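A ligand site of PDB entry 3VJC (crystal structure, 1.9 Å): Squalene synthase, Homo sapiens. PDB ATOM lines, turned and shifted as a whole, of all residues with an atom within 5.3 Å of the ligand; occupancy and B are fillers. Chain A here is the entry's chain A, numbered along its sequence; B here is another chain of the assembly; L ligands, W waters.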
ATOM      1  N   THR A  23      13.386 -31.113 -10.772  1.00  0.00           N
ATOM      2  CA  THR A  23      13.623 -30.101  -9.751  1.00  0.00           C
ATOM      3  C   THR A  23      12.356 -29.645  -9.018  1.00  0.00           C
ATOM      4  O   THR A  23      12.363 -29.458  -7.804  1.00  0.00           O
ATOM      5  CB  THR A  23      14.426 -28.888 -10.297  1.00  0.00           C
ATOM      6  OG1 THR A  23      13.687 -28.224 -11.322  1.00  0.00           O
ATOM      7  CG2 THR A  23      15.733 -29.383 -10.905  1.00  0.00           C
ATOM      8  N   SER A  24      11.256 -29.489  -9.731  1.00  0.00           N
ATOM      9  CA  SER A  24      10.052 -28.904  -9.151  1.00  0.00           C
ATOM     10  C   SER A  24       8.997 -29.963  -8.831  1.00  0.00           C
ATOM     11  O   SER A  24       8.432 -30.559  -9.758  1.00  0.00           O
ATOM     12  CB  SER A  24       9.456 -27.880 -10.131  1.00  0.00           C
ATOM     13  OG  SER A  24       8.274 -27.285  -9.595  1.00  0.00           O
ATOM     14  N   ARG A  25       8.703 -30.177  -7.557  1.00  0.00           N
ATOM     15  CA  ARG A  25       7.581 -31.057  -7.189  1.00  0.00           C
ATOM     16  C   ARG A  25       6.243 -30.344  -7.259  1.00  0.00           C
ATOM     17  O   ARG A  25       5.220 -30.991  -7.530  1.00  0.00           O
ATOM     18  CB  ARG A  25       7.769 -31.663  -5.799  1.00  0.00           C
ATOM     19  CG  ARG A  25       8.957 -32.612  -5.679  1.00  0.00           C
ATOM     20  CD  ARG A  25       9.253 -32.887  -4.205  1.00  0.00           C
ATOM     21  NE  ARG A  25       9.751 -31.701  -3.520  1.00  0.00           N
ATOM     22  CZ  ARG A  25      10.029 -31.622  -2.218  1.00  0.00           C
ATOM     23  NH1 ARG A  25      10.484 -30.490  -1.700  1.00  0.00           N
ATOM     24  NH2 ARG A  25       9.839 -32.660  -1.417  1.00  0.00           N
ATOM     25  N   SER A  26       6.207 -29.038  -7.042  1.00  0.00           N
ATOM     26  CA  SER A  26       4.932 -28.359  -6.871  1.00  0.00           C
ATOM     27  C   SER A  26       4.553 -27.325  -7.931  1.00  0.00           C
ATOM     28  O   SER A  26       3.407 -26.913  -7.921  1.00  0.00           O
ATOM     29  CB  SER A  26       4.822 -27.708  -5.490  1.00  0.00           C
ATOM     30  OG  SER A  26       4.935 -28.691  -4.468  1.00  0.00           O
ATOM     31  N   PHE A  27       5.497 -26.834  -8.743  1.00  0.00           N
ATOM     32  CA  PHE A  27       5.152 -25.898  -9.813  1.00  0.00           C
ATOM     33  C   PHE A  27       5.066 -26.542 -11.208  1.00  0.00           C
ATOM     34  O   PHE A  27       4.404 -25.997 -12.091  1.00  0.00           O
ATOM     35  CB  PHE A  27       6.170 -24.736  -9.898  1.00  0.00           C
ATOM     36  CG  PHE A  27       5.937 -23.648  -8.897  1.00  0.00           C
ATOM     37  CD1 PHE A  27       6.866 -23.421  -7.885  1.00  0.00           C
ATOM     38  CD2 PHE A  27       4.837 -22.808  -9.011  1.00  0.00           C
ATOM     39  CE1 PHE A  27       6.700 -22.382  -6.984  1.00  0.00           C
ATOM     40  CE2 PHE A  27       4.638 -21.776  -8.084  1.00  0.00           C
ATOM     41  CZ  PHE A  27       5.572 -21.566  -7.087  1.00  0.00           C
ATOM     42  N   ILE A  31       2.757 -25.228 -14.337  1.00  0.00           N
ATOM     43  CA  ILE A  31       3.466 -24.640 -15.483  1.00  0.00           C
ATOM     44  C   ILE A  31       3.128 -25.364 -16.790  1.00  0.00           C
ATOM     45  O   ILE A  31       2.837 -24.723 -17.812  1.00  0.00           O
ATOM     46  CB  ILE A  31       4.999 -24.585 -15.250  1.00  0.00           C
ATOM     47  CG1 ILE A  31       5.328 -23.607 -14.113  1.00  0.00           C
ATOM     48  CG2 ILE A  31       5.760 -24.249 -16.531  1.00  0.00           C
ATOM     49  CD1 ILE A  31       6.800 -23.675 -13.586  1.00  0.00           C
ATOM     50  N   VAL A  42       7.494 -19.923 -19.332  1.00  0.00           N
ATOM     51  CA  VAL A  42       7.581 -20.094 -17.886  1.00  0.00           C
ATOM     52  C   VAL A  42       8.442 -21.288 -17.464  1.00  0.00           C
ATOM     53  O   VAL A  42       9.170 -21.238 -16.479  1.00  0.00           O
ATOM     54  CB  VAL A  42       6.164 -20.085 -17.248  1.00  0.00           C
ATOM     55  CG1 VAL A  42       6.214 -20.296 -15.745  1.00  0.00           C
ATOM     56  CG2 VAL A  42       5.441 -18.749 -17.528  1.00  0.00           C
ATOM     57  N   PHE A  45      11.836 -19.796 -17.788  1.00  0.00           N
ATOM     58  CA  PHE A  45      12.052 -18.841 -16.705  1.00  0.00           C
ATOM     59  C   PHE A  45      12.327 -19.560 -15.379  1.00  0.00           C
ATOM     60  O   PHE A  45      13.241 -19.174 -14.634  1.00  0.00           O
ATOM     61  CB  PHE A  45      10.820 -17.947 -16.530  1.00  0.00           C
ATOM     62  CG  PHE A  45      11.018 -16.749 -15.635  1.00  0.00           C
ATOM     63  CD1 PHE A  45      12.217 -16.052 -15.569  1.00  0.00           C
ATOM     64  CD2 PHE A  45       9.921 -16.265 -14.916  1.00  0.00           C
ATOM     65  CE1 PHE A  45      12.338 -14.883 -14.791  1.00  0.00           C
ATOM     66  CE2 PHE A  45      10.022 -15.106 -14.134  1.00  0.00           C
ATOM     67  CZ  PHE A  45      11.234 -14.414 -14.065  1.00  0.00           C
ATOM     68  N   TYR A  46      11.523 -20.588 -15.088  1.00  0.00           N
ATOM     69  CA  TYR A  46      11.758 -21.422 -13.910  1.00  0.00           C
ATOM     70  C   TYR A  46      13.191 -21.990 -13.876  1.00  0.00           C
ATOM     71  O   TYR A  46      13.898 -21.894 -12.859  1.00  0.00           O
ATOM     72  CB  TYR A  46      10.733 -22.573 -13.839  1.00  0.00           C
ATOM     73  CG  TYR A  46      10.850 -23.363 -12.551  1.00  0.00           C
ATOM     74  CD1 TYR A  46      11.859 -24.309 -12.387  1.00  0.00           C
ATOM     75  CD2 TYR A  46      10.008 -23.106 -11.472  1.00  0.00           C
ATOM     76  CE1 TYR A  46      12.018 -24.994 -11.206  1.00  0.00           C
ATOM     77  CE2 TYR A  46      10.150 -23.818 -10.261  1.00  0.00           C
ATOM     78  CZ  TYR A  46      11.179 -24.739 -10.144  1.00  0.00           C
ATOM     79  OH  TYR A  46      11.362 -25.461  -8.989  1.00  0.00           O
ATOM     80  N   LEU A  49      15.940 -19.264 -13.388  1.00  0.00           N
ATOM     81  CA  LEU A  49      15.971 -18.775 -12.013  1.00  0.00           C
ATOM     82  C   LEU A  49      16.416 -19.858 -11.053  1.00  0.00           C
ATOM     83  O   LEU A  49      17.063 -19.585 -10.046  1.00  0.00           O
ATOM     84  CB  LEU A  49      14.617 -18.205 -11.582  1.00  0.00           C
ATOM     85  CG  LEU A  49      14.177 -16.906 -12.273  1.00  0.00           C
ATOM     86  CD1 LEU A  49      12.931 -16.429 -11.562  1.00  0.00           C
ATOM     87  CD2 LEU A  49      15.245 -15.817 -12.263  1.00  0.00           C
ATOM     88  N   ARG A  50      16.079 -21.113 -11.345  1.00  0.00           N
ATOM     89  CA  ARG A  50      16.574 -22.220 -10.540  1.00  0.00           C
ATOM     90  C   ARG A  50      18.117 -22.300 -10.536  1.00  0.00           C
ATOM     91  O   ARG A  50      18.750 -22.554  -9.512  1.00  0.00           O
ATOM     92  CB  ARG A  50      15.967 -23.524 -11.053  1.00  0.00           C
ATOM     93  CG  ARG A  50      16.259 -24.695 -10.146  1.00  0.00           C
ATOM     94  CD  ARG A  50      15.248 -24.684  -9.013  1.00  0.00           C
ATOM     95  NE  ARG A  50      15.693 -25.481  -7.878  1.00  0.00           N
ATOM     96  CZ  ARG A  50      14.869 -26.089  -7.040  1.00  0.00           C
ATOM     97  NH1 ARG A  50      13.561 -26.029  -7.253  1.00  0.00           N
ATOM     98  NH2 ARG A  50      15.345 -26.789  -6.012  1.00  0.00           N
ATOM     99  N   ASP A  53      19.368 -19.431  -8.406  1.00  0.00           N
ATOM    100  CA  ASP A  53      19.143 -19.798  -7.011  1.00  0.00           C
ATOM    101  C   ASP A  53      20.181 -20.783  -6.470  1.00  0.00           C
ATOM    102  O   ASP A  53      20.665 -20.624  -5.354  1.00  0.00           O
ATOM    103  CB  ASP A  53      17.721 -20.354  -6.852  1.00  0.00           C
ATOM    104  CG  ASP A  53      17.415 -20.748  -5.420  1.00  0.00           C
ATOM    105  OD1 ASP A  53      17.446 -21.956  -5.083  1.00  0.00           O
ATOM    106  OD2 ASP A  53      17.167 -19.836  -4.612  1.00  0.00           O
ATOM    107  N   LYS A  90      22.257 -29.991  -4.826  1.00  0.00           N
ATOM    108  CA  LYS A  90      21.459 -31.105  -5.339  1.00  0.00           C
ATOM    109  C   LYS A  90      20.872 -30.850  -6.728  1.00  0.00           C
ATOM    110  O   LYS A  90      20.660 -31.797  -7.480  1.00  0.00           O
ATOM    111  CB  LYS A  90      20.368 -31.523  -4.338  1.00  0.00           C
ATOM    112  CG  LYS A  90      19.180 -30.574  -4.228  1.00  0.00           C
ATOM    113  CD  LYS A  90      18.310 -30.869  -3.007  1.00  0.00           C
ATOM    114  CE  LYS A  90      16.852 -30.519  -3.260  1.00  0.00           C
ATOM    115  NZ  LYS A  90      16.647 -29.091  -3.651  1.00  0.00           N
ATOM    116  N   ASP A  91      20.633 -29.587  -7.075  1.00  0.00           N
ATOM    117  CA  ASP A  91      20.020 -29.220  -8.364  1.00  0.00           C
ATOM    118  C   ASP A  91      21.025 -28.780  -9.425  1.00  0.00           C
ATOM    119  O   ASP A  91      20.684 -28.126 -10.411  1.00  0.00           O
ATOM    120  CB  ASP A  91      18.961 -28.136  -8.152  1.00  0.00           C
ATOM    121  CG  ASP A  91      17.853 -28.595  -7.214  1.00  0.00           C
ATOM    122  OD1 ASP A  91      17.189 -29.599  -7.552  1.00  0.00           O
ATOM    123  OD2 ASP A  91      17.701 -27.996  -6.136  1.00  0.00           O
ATOM    124  N   MET A 123      17.774  -9.515 -10.247  1.00  0.00           N
ATOM    125  CA  MET A 123      17.888 -10.483  -9.174  1.00  0.00           C
ATOM    126  C   MET A 123      19.340 -10.774  -8.764  1.00  0.00           C
ATOM    127  O   MET A 123      19.655 -10.887  -7.574  1.00  0.00           O
ATOM    128  CB  MET A 123      17.190 -11.801  -9.554  1.00  0.00           C
ATOM    129  CG  MET A 123      17.206 -12.864  -8.446  1.00  0.00           C
ATOM    130  SD  MET A 123      16.112 -14.271  -8.804  1.00  0.00           S
ATOM    131  CE  MET A 123      14.677 -13.363  -9.396  1.00  0.00           C
ATOM    132  N   MET A 127      20.737 -10.420  -5.086  1.00  0.00           N
ATOM    133  CA  MET A 127      21.285 -11.591  -4.410  1.00  0.00           C
ATOM    134  C   MET A 127      22.707 -11.309  -3.960  1.00  0.00           C
ATOM    135  O   MET A 127      23.096 -11.697  -2.840  1.00  0.00           O
ATOM    136  CB  MET A 127      21.254 -12.812  -5.331  1.00  0.00           C
ATOM    137  CG  MET A 127      19.840 -13.400  -5.527  1.00  0.00           C
ATOM    138  SD  MET A 127      20.039 -14.766  -6.707  1.00  0.00           S
ATOM    139  CE  MET A 127      18.563 -15.733  -6.393  1.00  0.00           C
ATOM    140  N   VAL A 148      14.437 -11.946  -4.356  1.00  0.00           N
ATOM    141  CA  VAL A 148      14.422 -13.391  -4.583  1.00  0.00           C
ATOM    142  C   VAL A 148      13.022 -13.928  -4.884  1.00  0.00           C
ATOM    143  O   VAL A 148      12.878 -15.106  -5.180  1.00  0.00           O
ATOM    144  CB  VAL A 148      15.107 -14.203  -3.436  1.00  0.00           C
ATOM    145  CG1 VAL A 148      16.537 -13.688  -3.169  1.00  0.00           C
ATOM    146  CG2 VAL A 148      14.266 -14.171  -2.134  1.00  0.00           C
ATOM    147  N   VAL A 152      10.307 -12.396  -9.145  1.00  0.00           N
ATOM    148  CA  VAL A 152       9.716 -13.544  -9.834  1.00  0.00           C
ATOM    149  C   VAL A 152       8.273 -13.246 -10.202  1.00  0.00           C
ATOM    150  O   VAL A 152       7.868 -13.500 -11.351  1.00  0.00           O
ATOM    151  CB  VAL A 152       9.829 -14.837  -8.992  1.00  0.00           C
ATOM    152  CG1 VAL A 152       9.261 -16.051  -9.758  1.00  0.00           C
ATOM    153  CG2 VAL A 152      11.302 -15.036  -8.619  1.00  0.00           C
ATOM    154  N   LEU A 156       6.870 -12.993 -14.018  1.00  0.00           N
ATOM    155  CA  LEU A 156       5.767 -13.850 -14.460  1.00  0.00           C
ATOM    156  C   LEU A 156       4.615 -13.015 -15.027  1.00  0.00           C
ATOM    157  O   LEU A 156       4.082 -13.297 -16.100  1.00  0.00           O
ATOM    158  CB  LEU A 156       5.255 -14.750 -13.315  1.00  0.00           C
ATOM    159  CG  LEU A 156       6.254 -15.849 -12.962  1.00  0.00           C
ATOM    160  CD1 LEU A 156       5.930 -16.451 -11.596  1.00  0.00           C
ATOM    161  CD2 LEU A 156       6.262 -16.930 -14.083  1.00  0.00           C
ATOM    162  N   LEU A 184       4.498 -15.259  -0.670  1.00  0.00           N
ATOM    163  CA  LEU A 184       4.952 -16.645  -0.747  1.00  0.00           C
ATOM    164  C   LEU A 184       6.280 -16.803  -0.022  1.00  0.00           C
ATOM    165  O   LEU A 184       6.474 -17.736   0.736  1.00  0.00           O
ATOM    166  CB  LEU A 184       5.113 -17.105  -2.203  1.00  0.00           C
ATOM    167  CG  LEU A 184       3.828 -17.181  -3.033  1.00  0.00           C
ATOM    168  CD1 LEU A 184       4.101 -17.928  -4.343  1.00  0.00           C
ATOM    169  CD2 LEU A 184       2.650 -17.838  -2.290  1.00  0.00           C
ATOM    170  N   GLN A 185       7.176 -15.828  -0.224  1.00  0.00           N
ATOM    171  CA  GLN A 185       8.527 -15.950   0.299  1.00  0.00           C
ATOM    172  C   GLN A 185       8.551 -15.793   1.822  1.00  0.00           C
ATOM    173  O   GLN A 185       9.266 -16.541   2.510  1.00  0.00           O
ATOM    174  CB  GLN A 185       9.421 -14.907  -0.356  1.00  0.00           C
ATOM    175  CG  GLN A 185      10.910 -15.047   0.012  1.00  0.00           C
ATOM    176  CD  GLN A 185      11.485 -16.359  -0.496  1.00  0.00           C
ATOM    177  OE1 GLN A 185      11.601 -16.576  -1.689  1.00  0.00           O
ATOM    178  NE2 GLN A 185      11.852 -17.240   0.400  1.00  0.00           N
ATOM    179  N   THR A 187       6.024 -16.449   3.802  1.00  0.00           N
ATOM    180  CA  THR A 187       5.425 -17.686   4.329  1.00  0.00           C
ATOM    181  C   THR A 187       6.463 -18.807   4.414  1.00  0.00           C
ATOM    182  O   THR A 187       6.565 -19.540   5.426  1.00  0.00           O
ATOM    183  CB  THR A 187       4.175 -18.110   3.503  1.00  0.00           C
ATOM    184  OG1 THR A 187       3.201 -17.063   3.587  1.00  0.00           O
ATOM    185  CG2 THR A 187       3.530 -19.362   4.071  1.00  0.00           C
ATOM    186  N   ASN A 188       7.209 -18.969   3.335  1.00  0.00           N
ATOM    187  CA  ASN A 188       8.249 -20.003   3.321  1.00  0.00           C
ATOM    188  C   ASN A 188       9.282 -19.787   4.406  1.00  0.00           C
ATOM    189  O   ASN A 188       9.685 -20.752   5.041  1.00  0.00           O
ATOM    190  CB  ASN A 188       9.005 -20.016   1.982  1.00  0.00           C
ATOM    191  CG  ASN A 188       8.219 -20.739   0.901  1.00  0.00           C
ATOM    192  OD1 ASN A 188       7.607 -21.775   1.151  1.00  0.00           O
ATOM    193  ND2 ASN A 188       8.265 -20.203  -0.313  1.00  0.00           N
ATOM    194  N   ARG A 191       7.763 -20.608   7.876  1.00  0.00           N
ATOM    195  CA  ARG A 191       7.565 -22.056   8.030  1.00  0.00           C
ATOM    196  C   ARG A 191       8.891 -22.801   8.232  1.00  0.00           C
ATOM    197  O   ARG A 191       8.939 -23.759   9.008  1.00  0.00           O
ATOM    198  CB  ARG A 191       6.852 -22.641   6.797  1.00  0.00           C
ATOM    199  CG  ARG A 191       6.527 -24.142   6.911  1.00  0.00           C
ATOM    200  CD  ARG A 191       6.207 -24.805   5.558  1.00  0.00           C
ATOM    201  NE  ARG A 191       7.316 -24.685   4.622  1.00  0.00           N
ATOM    202  CZ  ARG A 191       7.215 -24.666   3.288  1.00  0.00           C
ATOM    203  NH1 ARG A 191       8.312 -24.530   2.561  1.00  0.00           N
ATOM    204  NH2 ARG A 191       6.043 -24.769   2.689  1.00  0.00           N
ATOM    205  N   PHE A 261      -2.455 -21.296 -11.926  1.00  0.00           N
ATOM    206  CA  PHE A 261      -1.035 -21.144 -11.614  1.00  0.00           C
ATOM    207  C   PHE A 261      -0.793 -20.111 -10.512  1.00  0.00           C
ATOM    208  O   PHE A 261       0.046 -20.322  -9.633  1.00  0.00           O
ATOM    209  CB  PHE A 261      -0.252 -20.813 -12.897  1.00  0.00           C
ATOM    210  CG  PHE A 261       1.183 -20.402 -12.656  1.00  0.00           C
ATOM    211  CD1 PHE A 261       2.198 -21.353 -12.526  1.00  0.00           C
ATOM    212  CD2 PHE A 261       1.503 -19.059 -12.479  1.00  0.00           C
ATOM    213  CE1 PHE A 261       3.533 -20.964 -12.289  1.00  0.00           C
ATOM    214  CE2 PHE A 261       2.826 -18.669 -12.220  1.00  0.00           C
ATOM    215  CZ  PHE A 261       3.838 -19.625 -12.120  1.00  0.00           C
ATOM    216  N   PRO A 265      -0.953 -21.435  -5.380  1.00  0.00           N
ATOM    217  CA  PRO A 265       0.107 -21.231  -4.401  1.00  0.00           C
ATOM    218  C   PRO A 265      -0.248 -20.200  -3.337  1.00  0.00           C
ATOM    219  O   PRO A 265       0.184 -20.328  -2.206  1.00  0.00           O
ATOM    220  CB  PRO A 265       1.318 -20.764  -5.237  1.00  0.00           C
ATOM    221  CG  PRO A 265       1.061 -21.379  -6.614  1.00  0.00           C
ATOM    222  CD  PRO A 265      -0.457 -21.179  -6.759  1.00  0.00           C
ATOM    223  N   MET A 268      -2.442 -21.962  -0.817  1.00  0.00           N
ATOM    224  CA  MET A 268      -1.638 -22.886  -0.037  1.00  0.00           C
ATOM    225  C   MET A 268      -0.779 -22.146   0.990  1.00  0.00           C
ATOM    226  O   MET A 268      -0.564 -22.665   2.078  1.00  0.00           O
ATOM    227  CB  MET A 268      -0.771 -23.729  -0.960  1.00  0.00           C
ATOM    228  CG  MET A 268      -1.627 -24.712  -1.737  1.00  0.00           C
ATOM    229  SD  MET A 268      -0.637 -25.673  -2.882  1.00  0.00           S
ATOM    230  CE  MET A 268       0.268 -26.746  -1.751  1.00  0.00           C
ATOM    231  N   ALA A 269      -0.280 -20.961   0.641  1.00  0.00           N
ATOM    232  CA  ALA A 269       0.511 -20.150   1.582  1.00  0.00           C
ATOM    233  C   ALA A 269      -0.385 -19.650   2.697  1.00  0.00           C
ATOM    234  O   ALA A 269       0.011 -19.669   3.860  1.00  0.00           O
ATOM    235  CB  ALA A 269       1.197 -18.970   0.883  1.00  0.00           C
ATOM    236  N   THR A 272      -0.956 -22.400   4.966  1.00  0.00           N
ATOM    237  CA  THR A 272       0.283 -22.609   5.729  1.00  0.00           C
ATOM    238  C   THR A 272       0.421 -21.611   6.887  1.00  0.00           C
ATOM    239  O   THR A 272       0.740 -22.002   8.001  1.00  0.00           O
ATOM    240  CB  THR A 272       1.501 -22.511   4.786  1.00  0.00           C
ATOM    241  OG1 THR A 272       1.435 -23.609   3.855  1.00  0.00           O
ATOM    242  CG2 THR A 272       2.795 -22.609   5.562  1.00  0.00           C
ATOM    243  N   VAL B 295      -0.676 -29.755  -4.368  1.00  0.00           N
ATOM    244  CA  VAL B 295      -1.092 -28.731  -5.321  1.00  0.00           C
ATOM    245  C   VAL B 295      -2.407 -29.087  -6.020  1.00  0.00           C
ATOM    246  O   VAL B 295      -3.250 -28.205  -6.239  1.00  0.00           O
ATOM    247  CB  VAL B 295       0.032 -28.375  -6.331  1.00  0.00           C
ATOM    248  CG1 VAL B 295      -0.317 -27.132  -7.139  1.00  0.00           C
ATOM    249  CG2 VAL B 295       1.322 -28.117  -5.583  1.00  0.00           C
HETATM  250  C1  LIG L   1      14.285 -21.612  -6.790  1.00  0.00           C
HETATM  251  C2  LIG L   1       3.743 -22.272   1.144  1.00  0.00           C
HETATM  252  C3  LIG L   1      14.727 -17.236  -7.054  1.00  0.00           C
HETATM  253  C4  LIG L   1       2.583 -24.808  -4.596  1.00  0.00           C
HETATM  254  C5  LIG L   1       4.158 -21.455  -1.824  1.00  0.00           C
HETATM  255  C6  LIG L   1      12.488 -21.132  -9.802  1.00  0.00           C
HETATM  256  O1  LIG L   1      13.272 -18.529  -5.635  1.00  0.00           O
HETATM  257  O2  LIG L   1       7.139 -25.944  -2.964  1.00  0.00           O
HETATM  258  O3  LIG L   1      14.090 -27.361  -3.460  1.00  0.00           O
HETATM  259  O4  LIG L   1       9.327 -28.196  -3.299  1.00  0.00           O
HETATM  260  O5  LIG L   1       8.247 -27.244  -6.145  1.00  0.00           O
HETATM  261  O6  LIG L   1      12.517 -28.802  -2.950  1.00  0.00           O
HETATM  262  O7  LIG L   1      10.125 -29.364  -4.962  1.00  0.00           O
HETATM  263  O8  LIG L   1       9.114 -25.864  -7.593  1.00  0.00           O
HETATM  264  O9  LIG L   1      10.874 -24.038  -2.504  1.00  0.00           O
HETATM  265  O10 LIG L   1      11.618 -27.590  -5.914  1.00  0.00           O
HETATM  266  C7  LIG L   1       5.840 -24.268  -4.043  1.00  0.00           C
HETATM  267  C8  LIG L   1       4.711 -24.655  -3.462  1.00  0.00           C
HETATM  268  C9  LIG L   1       7.697 -20.186 -12.038  1.00  0.00           C
HETATM  269  C10 LIG L   1       8.926 -19.649 -12.437  1.00  0.00           C
HETATM  270  C11 LIG L   1       7.466 -20.452 -10.686  1.00  0.00           C
HETATM  271  C12 LIG L   1       9.921 -19.417 -11.497  1.00  0.00           C
HETATM  272  C13 LIG L   1       8.469 -20.230  -9.731  1.00  0.00           C
HETATM  273  C14 LIG L   1       2.881 -22.702  -0.030  1.00  0.00           C
HETATM  274  C15 LIG L   1      11.974 -22.224  -5.900  1.00  0.00           C
HETATM  275  C16 LIG L   1      12.669 -23.376  -5.193  1.00  0.00           C
HETATM  276  C17 LIG L   1      10.814 -19.412  -9.163  1.00  0.00           C
HETATM  277  C18 LIG L   1       2.765 -23.516  -2.409  1.00  0.00           C
HETATM  278  O11 LIG L   1      13.302 -19.230  -7.789  1.00  0.00           O
HETATM  279  O12 LIG L   1       8.232 -24.553  -4.497  1.00  0.00           O
HETATM  280  O13 LIG L   1      12.534 -25.484  -4.168  1.00  0.00           O
HETATM  281  O14 LIG L   1      11.017 -25.043  -5.846  1.00  0.00           O
HETATM  282  C19 LIG L   1      13.750 -18.335  -6.738  1.00  0.00           C
HETATM  283  C20 LIG L   1       7.079 -25.014  -3.768  1.00  0.00           C
HETATM  284  C21 LIG L   1      12.957 -21.375  -6.721  1.00  0.00           C
HETATM  285  C22 LIG L   1      12.883 -27.672  -3.352  1.00  0.00           C
HETATM  286  C23 LIG L   1      10.045 -28.294  -4.314  1.00  0.00           C
HETATM  287  C24 LIG L   1       9.083 -26.356  -6.436  1.00  0.00           C
HETATM  288  C25 LIG L   1       9.701 -19.718 -10.150  1.00  0.00           C
HETATM  289  C26 LIG L   1       3.442 -23.883  -3.728  1.00  0.00           C
HETATM  290  C27 LIG L   1       3.636 -22.815  -1.362  1.00  0.00           C
HETATM  291  C28 LIG L   1      11.571 -20.641  -8.684  1.00  0.00           C
HETATM  292  C29 LIG L   1      10.520 -24.061  -3.885  1.00  0.00           C
HETATM  293  C30 LIG L   1      12.328 -20.213  -7.428  1.00  0.00           C
HETATM  294  C31 LIG L   1      11.842 -26.644  -3.710  1.00  0.00           C
HETATM  295  C32 LIG L   1       9.479 -25.158  -4.161  1.00  0.00           C
HETATM  296  C33 LIG L   1      10.870 -27.126  -4.797  1.00  0.00           C
HETATM  297  C34 LIG L   1      11.711 -24.467  -4.745  1.00  0.00           C
HETATM  298  C35 LIG L   1      10.049 -25.946  -5.346  1.00  0.00           C
HETATM  299  O   HOH W   1      12.883 -31.097  -4.785  1.00  0.00           O
HETATM  300  O   HOH W   2      13.062 -24.917  -0.902  1.00  0.00           O
HETATM  301  O   HOH W   3       6.990 -29.165  -3.019  1.00  0.00           O
HETATM  302  O   HOH W   4      13.301 -28.797  -0.381  1.00  0.00           O
HETATM  303  O   HOH W   5      16.456 -17.350  -4.042  1.00  0.00           O
HETATM  304  O   HOH W   6       6.179 -27.798  -0.804  1.00  0.00           O
HETATM  305  O   HOH W   7      13.722 -17.384  -3.143  1.00  0.00           O
HETATM  306  O   HOH W   8      15.158 -25.089  -2.897  1.00  0.00           O
HETATM  307  O   HOH W   9      14.253 -20.241  -3.421  1.00  0.00           O
HETATM  308  O   HOH W  10       9.110 -27.278  -0.882  1.00  0.00           O
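N of Ser 26 lies within hydrogen-bond range of O5 of the ligand, 2.9 Å away. NH2 of Arg 50 is in salt-bridge range of O3 of the ligand, 2.9 Å away. NZ of Lys 90 lies within salt-bridge range of O3 of the ligand (3.1 Å). The side-chain hydroxyl (OG) of Ser 24 lies within hydrogen-bond range of an oxygen (O8) of the ligand (2.6 Å). The backbone carbonyl oxygen (O) of Thr 23 is in hydrogen-bond range of an oxygen (O10) of the ligand (2.8 Å). N of Arg 25 sits at hydrogen-bond distance from O7 of the ligand (3.1 Å). The side-chain hydroxyl of Tyr 46 sits at hydrogen-bond distance from an oxygen (O8) of the ligand (2.7 Å). NE of Arg 25 lies within salt-bridge range of O7 of the ligand, at 2.8 Å.
The side-chain amide nitrogen (ND2) of Asn 188 is in hydrogen-bond range of the backbone carbonyl oxygen (O) of Leu 184 (3.2 Å). The side-chain hydroxyl of Thr 272 sits at hydrogen-bond distance from the backbone carbonyl oxygen of Met 268 (2.8 Å). The side-chain carboxylate (OD2) of Asp 91 is in salt-bridge range of the side-chain amino group (NZ) of Lys 90, at 2.9 Å. OG of Ser 24 sits at hydrogen-bond distance from N of Phe 27 (2.9 Å). The side-chain hydroxyl (OH) of Tyr 46 sits at hydrogen-bond distance from the guanidinium group (NH1) of Arg 50, at 2.9 Å. NH2 of Arg 50 is in salt-bridge range of OD2 of Asp 91, at 2.7 Å. The side-chain amide oxygen of Asn 188 is in hydrogen-bond range of the guanidinium group of Arg 191 (3.2 Å).
The backbone carbonyl oxygen (O) of Val 148 sits close to an oxygen (O1) of the ligand (3.5 Å). Residues that only touch the ligand: Phe 27, Ile 31, Val 42, Asp 53, Met 123, Val 152, Leu 184, Asn 188, Arg 191, Phe 261, Met 268, Ala 269, Thr 272 and Val 295 of chain B. Hydrophobic or aromatic side chains that line the ligand: Phe 27, Ile 31, Val 42, Tyr 46, Met 123, Val 152, Leu 184, Phe 261, Met 268 and Val 295 of chain B. Of the 30 residues printed, 22 come within 4 Å of the ligand.
Water W3 lies within hydrogen-bond range of an oxygen (O4) of the ligand and the side-chain hydroxyl (OG) of Ser 26. Water W1 lies within hydrogen-bond range of an oxygen (O6) of the ligand (3.0 Å), the guanidinium group of Arg 25 (3.4 Å) and the backbone carbonyl oxygen of Thr 23 (3.5 Å). Water W9 lies within hydrogen-bond range of an oxygen (O1) of the ligand (3.0 Å) and the side-chain carboxylate of Asp 53 (3.2 Å).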
